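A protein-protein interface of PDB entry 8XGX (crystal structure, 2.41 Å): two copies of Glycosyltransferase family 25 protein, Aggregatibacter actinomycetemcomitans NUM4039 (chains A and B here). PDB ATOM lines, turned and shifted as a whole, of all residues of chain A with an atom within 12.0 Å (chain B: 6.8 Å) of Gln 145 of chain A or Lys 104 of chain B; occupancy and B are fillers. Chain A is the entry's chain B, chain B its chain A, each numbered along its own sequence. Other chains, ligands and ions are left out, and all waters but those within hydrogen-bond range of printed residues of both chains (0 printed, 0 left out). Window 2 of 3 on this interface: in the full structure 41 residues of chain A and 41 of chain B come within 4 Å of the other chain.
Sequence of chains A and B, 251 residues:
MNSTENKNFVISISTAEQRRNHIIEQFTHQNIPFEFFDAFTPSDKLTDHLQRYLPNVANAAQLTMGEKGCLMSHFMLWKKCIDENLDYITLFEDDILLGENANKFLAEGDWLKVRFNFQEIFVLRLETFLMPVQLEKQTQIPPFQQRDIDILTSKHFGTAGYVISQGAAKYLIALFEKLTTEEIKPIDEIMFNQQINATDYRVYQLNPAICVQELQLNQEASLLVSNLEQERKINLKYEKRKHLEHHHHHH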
ATOM      1  N   ILE A 141       7.201  25.750  15.431  1.00  0.00           N
ATOM      2  CA  ILE A 141       7.941  26.442  16.526  1.00  0.00           C
ATOM      3  C   ILE A 141       9.441  26.231  16.350  1.00  0.00           C
ATOM      4  O   ILE A 141       9.943  25.126  16.513  1.00  0.00           O
ATOM      5  CB  ILE A 141       7.455  25.963  17.903  1.00  0.00           C
ATOM      6  CG1 ILE A 141       5.979  26.307  18.107  1.00  0.00           C
ATOM      7  CG2 ILE A 141       8.321  26.573  18.993  1.00  0.00           C
ATOM      8  CD1 ILE A 141       5.280  25.421  19.086  1.00  0.00           C
ATOM      9  N   PRO A 142      10.210  27.295  16.043  1.00  0.00           N
ATOM     10  CA  PRO A 142      11.625  27.143  15.729  1.00  0.00           C
ATOM     11  C   PRO A 142      12.497  26.749  16.920  1.00  0.00           C
ATOM     12  O   PRO A 142      12.202  27.090  18.068  1.00  0.00           O
ATOM     13  CB  PRO A 142      12.039  28.524  15.196  1.00  0.00           C
ATOM     14  CG  PRO A 142      11.014  29.486  15.748  1.00  0.00           C
ATOM     15  CD  PRO A 142       9.743  28.684  15.929  1.00  0.00           C
ATOM     16  N   PRO A 143      13.589  25.995  16.668  1.00  0.00           N
ATOM     17  CA  PRO A 143      14.561  25.661  17.700  1.00  0.00           C
ATOM     18  C   PRO A 143      15.206  26.895  18.344  1.00  0.00           C
ATOM     19  O   PRO A 143      15.101  27.970  17.793  1.00  0.00           O
ATOM     20  CB  PRO A 143      15.637  24.829  16.975  1.00  0.00           C
ATOM     21  CG  PRO A 143      15.400  25.080  15.501  1.00  0.00           C
ATOM     22  CD  PRO A 143      13.920  25.377  15.377  1.00  0.00           C
ATOM     23  N   PHE A 144      15.837  26.688  19.502  1.00  0.00           N
ATOM     24  CA  PHE A 144      16.514  27.727  20.315  1.00  0.00           C
ATOM     25  C   PHE A 144      17.769  27.124  20.938  1.00  0.00           C
ATOM     26  O   PHE A 144      17.665  26.017  21.481  1.00  0.00           O
ATOM     27  CB  PHE A 144      15.579  28.237  21.412  1.00  0.00           C
ATOM     28  CG  PHE A 144      16.202  29.247  22.340  1.00  0.00           C
ATOM     29  CD1 PHE A 144      16.741  30.424  21.843  1.00  0.00           C
ATOM     30  CD2 PHE A 144      16.232  29.033  23.708  1.00  0.00           C
ATOM     31  CE1 PHE A 144      17.292  31.366  22.701  1.00  0.00           C
ATOM     32  CE2 PHE A 144      16.781  29.976  24.563  1.00  0.00           C
ATOM     33  CZ  PHE A 144      17.318  31.138  24.059  1.00  0.00           C
ATOM     34  N   GLN A 145      18.900  27.829  20.849  1.00  0.00           N
ATOM     35  CA  GLN A 145      20.217  27.380  21.381  1.00  0.00           C
ATOM     36  C   GLN A 145      20.561  25.991  20.820  1.00  0.00           C
ATOM     37  O   GLN A 145      21.117  25.172  21.576  1.00  0.00           O
ATOM     38  CB  GLN A 145      20.164  27.391  22.909  1.00  0.00           C
ATOM     39  CG  GLN A 145      19.983  28.780  23.500  1.00  0.00           C
ATOM     40  CD  GLN A 145      21.279  29.559  23.541  1.00  0.00           C
ATOM     41  OE1 GLN A 145      21.310  30.780  23.366  1.00  0.00           O
ATOM     42  NE2 GLN A 145      22.373  28.855  23.779  1.00  0.00           N
ATOM     43  N   GLN A 146      20.197  25.743  19.553  1.00  0.00           N
ATOM     44  CA  GLN A 146      20.467  24.498  18.772  1.00  0.00           C
ATOM     45  C   GLN A 146      19.838  23.266  19.435  1.00  0.00           C
ATOM     46  O   GLN A 146      20.258  22.150  19.104  1.00  0.00           O
ATOM     47  CB  GLN A 146      21.972  24.317  18.576  1.00  0.00           C
ATOM     48  CG  GLN A 146      22.585  25.404  17.706  1.00  0.00           C
ATOM     49  CD  GLN A 146      23.988  25.746  18.131  1.00  0.00           C
ATOM     50  OE1 GLN A 146      24.261  26.016  19.303  1.00  0.00           O
ATOM     51  NE2 GLN A 146      24.892  25.740  17.166  1.00  0.00           N
ATOM     52  N   ARG A 147      18.834  23.455  20.292  1.00  0.00           N
ATOM     53  CA  ARG A 147      17.973  22.363  20.818  1.00  0.00           C
ATOM     54  C   ARG A 147      16.654  22.395  20.055  1.00  0.00           C
ATOM     55  O   ARG A 147      16.139  23.509  19.815  1.00  0.00           O
ATOM     56  CB  ARG A 147      17.724  22.537  22.314  1.00  0.00           C
ATOM     57  CG  ARG A 147      18.984  22.890  23.082  1.00  0.00           C
ATOM     58  CD  ARG A 147      18.927  22.334  24.481  1.00  0.00           C
ATOM     59  NE  ARG A 147      20.107  22.742  25.219  1.00  0.00           N
ATOM     60  CZ  ARG A 147      20.509  22.210  26.362  1.00  0.00           C
ATOM     61  NH1 ARG A 147      19.816  21.235  26.929  1.00  0.00           N
ATOM     62  NH2 ARG A 147      21.608  22.663  26.945  1.00  0.00           N
ATOM     63  N   ASP A 148      16.140  21.221  19.688  1.00  0.00           N
ATOM     64  CA  ASP A 148      14.819  21.093  19.025  1.00  0.00           C
ATOM     65  C   ASP A 148      13.721  21.225  20.081  1.00  0.00           C
ATOM     66  O   ASP A 148      13.976  20.980  21.276  1.00  0.00           O
ATOM     67  CB  ASP A 148      14.689  19.789  18.234  1.00  0.00           C
ATOM     68  CG  ASP A 148      15.731  19.645  17.129  1.00  0.00           C
ATOM     69  OD1 ASP A 148      15.883  20.607  16.342  1.00  0.00           O
ATOM     70  OD2 ASP A 148      16.408  18.592  17.089  1.00  0.00           O
ATOM     71  N   ILE A 149      12.557  21.661  19.625  1.00  0.00           N
ATOM     72  CA  ILE A 149      11.278  21.616  20.365  1.00  0.00           C
ATOM     73  C   ILE A 149      10.425  20.589  19.618  1.00  0.00           C
ATOM     74  O   ILE A 149       9.898  20.914  18.526  1.00  0.00           O
ATOM     75  CB  ILE A 149      10.677  23.032  20.441  1.00  0.00           C
ATOM     76  CG1 ILE A 149      11.626  23.962  21.198  1.00  0.00           C
ATOM     77  CG2 ILE A 149       9.289  23.022  21.056  1.00  0.00           C
ATOM     78  CD1 ILE A 149      11.176  25.389  21.242  1.00  0.00           C
ATOM     79  N   GLN B  30      23.607  29.907  38.613  1.00  0.00           N
ATOM     80  CA  GLN B  30      23.276  30.258  37.202  1.00  0.00           C
ATOM     81  C   GLN B  30      22.452  31.559  37.141  1.00  0.00           C
ATOM     82  O   GLN B  30      21.989  31.897  36.047  1.00  0.00           O
ATOM     83  CB  GLN B  30      22.562  29.084  36.532  1.00  0.00           C
ATOM     84  CG  GLN B  30      23.446  27.858  36.347  1.00  0.00           C
ATOM     85  CD  GLN B  30      22.949  26.961  35.236  1.00  0.00           C
ATOM     86  OE1 GLN B  30      22.546  27.424  34.170  1.00  0.00           O
ATOM     87  NE2 GLN B  30      22.963  25.656  35.472  1.00  0.00           N
ATOM     88  N   ILE B  32      19.450  32.453  38.170  1.00  0.00           N
ATOM     89  CA  ILE B  32      18.048  32.197  37.741  1.00  0.00           C
ATOM     90  C   ILE B  32      17.157  32.565  38.917  1.00  0.00           C
ATOM     91  O   ILE B  32      17.257  31.961  39.983  1.00  0.00           O
ATOM     92  CB  ILE B  32      17.861  30.730  37.313  1.00  0.00           C
ATOM     93  CG1 ILE B  32      18.818  30.344  36.181  1.00  0.00           C
ATOM     94  CG2 ILE B  32      16.407  30.454  36.958  1.00  0.00           C
ATOM     95  CD1 ILE B  32      18.963  28.859  35.990  1.00  0.00           C
ATOM     96  N   ASN B 101      23.904  25.892  31.140  1.00  0.00           N
ATOM     97  CA  ASN B 101      23.178  26.787  30.197  1.00  0.00           C
ATOM     98  C   ASN B 101      21.661  26.728  30.431  1.00  0.00           C
ATOM     99  O   ASN B 101      20.953  27.237  29.560  1.00  0.00           O
ATOM    100  CB  ASN B 101      23.468  26.478  28.720  1.00  0.00           C
ATOM    101  CG  ASN B 101      24.925  26.609  28.327  1.00  0.00           C
ATOM    102  OD1 ASN B 101      25.622  27.522  28.771  1.00  0.00           O
ATOM    103  ND2 ASN B 101      25.393  25.696  27.489  1.00  0.00           N
ATOM    104  N   ALA B 102      21.164  26.184  31.553  1.00  0.00           N
ATOM    105  CA  ALA B 102      19.727  26.243  31.915  1.00  0.00           C
ATOM    106  C   ALA B 102      19.291  27.711  32.018  1.00  0.00           C
ATOM    107  O   ALA B 102      18.134  28.016  31.680  1.00  0.00           O
ATOM    108  CB  ALA B 102      19.458  25.498  33.200  1.00  0.00           C
ATOM    109  N   ASN B 103      20.192  28.592  32.451  1.00  0.00           N
ATOM    110  CA  ASN B 103      19.914  30.038  32.657  1.00  0.00           C
ATOM    111  C   ASN B 103      19.540  30.709  31.329  1.00  0.00           C
ATOM    112  O   ASN B 103      18.779  31.690  31.378  1.00  0.00           O
ATOM    113  CB  ASN B 103      21.077  30.763  33.342  1.00  0.00           C
ATOM    114  CG  ASN B 103      22.423  30.538  32.686  1.00  0.00           C
ATOM    115  OD1 ASN B 103      22.530  29.877  31.652  1.00  0.00           O
ATOM    116  ND2 ASN B 103      23.465  31.078  33.298  1.00  0.00           N
ATOM    117  N   LYS B 104      20.032  30.199  30.198  1.00  0.00           N
ATOM    118  CA  LYS B 104      19.690  30.694  28.836  1.00  0.00           C
ATOM    119  C   LYS B 104      18.203  30.452  28.550  1.00  0.00           C
ATOM    120  O   LYS B 104      17.612  31.240  27.782  1.00  0.00           O
ATOM    121  CB  LYS B 104      20.567  30.024  27.777  1.00  0.00           C
ATOM    122  CG  LYS B 104      22.042  30.378  27.863  1.00  0.00           C
ATOM    123  CD  LYS B 104      22.811  29.885  26.665  1.00  0.00           C
ATOM    124  CE  LYS B 104      24.305  30.116  26.750  1.00  0.00           C
ATOM    125  NZ  LYS B 104      24.962  29.787  25.461  1.00  0.00           N
ATOM    126  N   PHE B 105      17.612  29.442  29.189  1.00  0.00           N
ATOM    127  CA  PHE B 105      16.173  29.089  29.067  1.00  0.00           C
ATOM    128  C   PHE B 105      15.358  29.663  30.225  1.00  0.00           C
ATOM    129  O   PHE B 105      14.190  29.984  29.981  1.00  0.00           O
ATOM    130  CB  PHE B 105      16.007  27.573  28.998  1.00  0.00           C
ATOM    131  CG  PHE B 105      16.752  26.966  27.842  1.00  0.00           C
ATOM    132  CD1 PHE B 105      18.113  26.732  27.928  1.00  0.00           C
ATOM    133  CD2 PHE B 105      16.104  26.669  26.661  1.00  0.00           C
ATOM    134  CE1 PHE B 105      18.813  26.196  26.861  1.00  0.00           C
ATOM    135  CE2 PHE B 105      16.805  26.131  25.595  1.00  0.00           C
ATOM    136  CZ  PHE B 105      18.156  25.898  25.695  1.00  0.00           C
ATOM    137  N   LEU B 106      15.942  29.791  31.419  1.00  0.00           N
ATOM    138  CA  LEU B 106      15.161  29.955  32.676  1.00  0.00           C
ATOM    139  C   LEU B 106      15.275  31.367  33.251  1.00  0.00           C
ATOM    140  O   LEU B 106      14.417  31.702  34.080  1.00  0.00           O
ATOM    141  CB  LEU B 106      15.648  28.920  33.694  1.00  0.00           C
ATOM    142  CG  LEU B 106      15.377  27.466  33.326  1.00  0.00           C
ATOM    143  CD1 LEU B 106      15.693  26.562  34.503  1.00  0.00           C
ATOM    144  CD2 LEU B 106      13.927  27.280  32.881  1.00  0.00           C
ATOM    145  N   ALA B 107      16.287  32.152  32.870  1.00  0.00           N
ATOM    146  CA  ALA B 107      16.489  33.539  33.365  1.00  0.00           C
ATOM    147  C   ALA B 107      15.508  34.484  32.667  1.00  0.00           C
ATOM    148  O   ALA B 107      14.901  35.309  33.369  1.00  0.00           O
ATOM    149  CB  ALA B 107      17.919  33.985  33.144  1.00  0.00           C
ATOM    150  N   GLU B 108      15.367  34.346  31.344  1.00  0.00           N
ATOM    151  CA  GLU B 108      14.637  35.286  30.449  1.00  0.00           C
ATOM    152  C   GLU B 108      13.536  34.502  29.718  1.00  0.00           C
ATOM    153  O   GLU B 108      13.728  33.291  29.491  1.00  0.00           O
ATOM    154  CB  GLU B 108      15.630  35.963  29.491  1.00  0.00           C
ATOM    155  CG  GLU B 108      15.011  36.956  28.494  1.00  0.00           C
ATOM    156  CD  GLU B 108      14.715  38.364  29.000  1.00  0.00           C
ATOM    157  OE1 GLU B 108      15.559  38.911  29.745  1.00  0.00           O
ATOM    158  OE2 GLU B 108      13.656  38.943  28.620  1.00  0.00           O
ATOM    159  N   GLY B 109      12.430  35.182  29.388  1.00  0.00           N
ATOM    160  CA  GLY B 109      11.254  34.620  28.700  1.00  0.00           C
ATOM    161  C   GLY B 109      11.165  35.034  27.238  1.00  0.00           C
ATOM    162  O   GLY B 109      10.203  34.613  26.582  1.00  0.00           O
ATOM    163  N   TRP B 111      12.750  34.165  24.490  1.00  0.00           N
ATOM    164  CA  TRP B 111      12.758  33.002  23.561  1.00  0.00           C
ATOM    165  C   TRP B 111      11.373  32.346  23.517  1.00  0.00           C
ATOM    166  O   TRP B 111      11.029  31.782  22.452  1.00  0.00           O
ATOM    167  CB  TRP B 111      13.848  32.001  23.946  1.00  0.00           C
ATOM    168  CG  TRP B 111      13.563  31.246  25.204  1.00  0.00           C
ATOM    169  CD1 TRP B 111      13.680  31.712  26.480  1.00  0.00           C
ATOM    170  CD2 TRP B 111      13.106  29.885  25.312  1.00  0.00           C
ATOM    171  NE1 TRP B 111      13.319  30.742  27.374  1.00  0.00           N
ATOM    172  CE2 TRP B 111      12.979  29.605  26.689  1.00  0.00           C
ATOM    173  CE3 TRP B 111      12.795  28.883  24.387  1.00  0.00           C
ATOM    174  CZ2 TRP B 111      12.548  28.365  27.160  1.00  0.00           C
ATOM    175  CZ3 TRP B 111      12.379  27.654  24.854  1.00  0.00           C
ATOM    176  CH2 TRP B 111      12.259  27.401  26.220  1.00  0.00           C
ATOM    177  N   ARG B 115       8.095  32.780  20.190  1.00  0.00           N
ATOM    178  CA  ARG B 115       7.735  31.444  19.640  1.00  0.00           C
ATOM    179  C   ARG B 115       6.257  31.106  19.886  1.00  0.00           C
ATOM    180  O   ARG B 115       5.678  30.364  19.061  1.00  0.00           O
ATOM    181  CB  ARG B 115       8.642  30.367  20.232  1.00  0.00           C
ATOM    182  CG  ARG B 115      10.044  30.381  19.645  1.00  0.00           C
ATOM    183  CD  ARG B 115      10.999  29.418  20.315  1.00  0.00           C
ATOM    184  NE  ARG B 115      12.259  29.441  19.593  1.00  0.00           N
ATOM    185  CZ  ARG B 115      13.173  30.401  19.692  1.00  0.00           C
ATOM    186  NH1 ARG B 115      12.993  31.433  20.505  1.00  0.00           N
ATOM    187  NH2 ARG B 115      14.278  30.320  18.973  1.00  0.00           N
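The side-chain amide nitrogen of Gln 145 of chain A sits close to the side-chain amino group of Lys 104 of chain B (3.2 Å). The guanidinium group of Arg 115 of chain B is in hydrogen-bond range of the backbone carbonyl oxygen of Pro 142 of chain A (2.8 Å). The guanidinium group of Arg 115 of chain B lies within hydrogen-bond range of the backbone carbonyl oxygen of Pro 143 of chain A, 2.8 Å away.
No position is printed for both chains. Of the 9 pairs that touch across the chains among the printed residues, none has its exchanged pair printed and touching as well.
Hydrophobic or aromatic side chains of chain B within 4 Å of the printed part of chain A: Phe 105 and Trp 111. Along chain B the printed residues that touch a printed residue of chain A span positions 104 to 115. Hydrophobic or aromatic side chains of chain A within 4 Å of the printed part of chain B: Phe 144. Among the printed residues, 9 pairs touch across the chains. Among the printed residues, no Asp or Glu carboxylate lies within 4 Å of a Lys or Arg side-chain nitrogen of the other chain.
Gln 145 of chain A touches just these residues of chain B: Lys 104 and Phe 105. Lys 104 of chain B touches just these residues of chain A: Phe 144 (3.6 Å) and Gln 145 (3.1 Å). No residue of chain A comes within 4 Å of Asn 101 of chain B. No residue of chain A comes within 4 Å of Ala 102 of chain B. Phe 105 of chain B touches just these residues of chain A: Phe 144, Gln 145 and Arg 147. No residue of chain A comes within 4 Å of Leu 106 of chain B. No residue of chain A comes within 4 Å of Ala 107 of chain B. Printed residues of chain B within 4 Å of Pro 142 of chain A: Arg 115 (2.8 Å). Of the printed residues of chain B, Pro 143 of chain A touches Arg 115. Of the printed residues of chain B, Phe 144 of chain A touches Lys 104 (3.6 Å), Phe 105 (3.5 Å), Trp 111 (3.5 Å) and Arg 115 (3.5 Å). Of the printed residues of chain A, Trp 111 of chain B touches Phe 144 (3.5 Å). The nearest residue of chain A that does not touch Lys 104 of chain B is Gln 146 of chain A (7.3 Å). The nearest printed residue of chain B that does not touch Arg 147 of chain A is Asn 101 of chain B (4.6 Å).
Phe 144 of chain A touches Lys 104 of chain B. CD2 of Phe 144 of chain A touches CE2 of Phe 105 of chain B (3.5 Å). CD2 of Phe 144 of chain A touches CE3 of Trp 111 of chain B (3.5 Å). Arg 115 of chain B touches Phe 144 of chain A (NH2 to CB, 3.5 Å). Phe 105 of chain B touches Gln 145 of chain A (CZ to CB, 3.7 Å). Phe 105 of chain B touches Arg 147 of chain A (CZ to NE, 3.7 Å).
The backbone carbonyl oxygen (O) of Glu 108 of chain B sits at hydrogen-bond distance from the indole nitrogen (NE1) of Trp 111 of chain B, at 3.3 Å. NH1 of Arg 115 of chain B is in hydrogen-bond range of O of Trp 111 of chain B. The indole nitrogen (NE1) of Trp 111 of chain B lies within hydrogen-bond range of the backbone carbonyl oxygen (O) of Phe 105 of chain B, 2.9 Å away.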
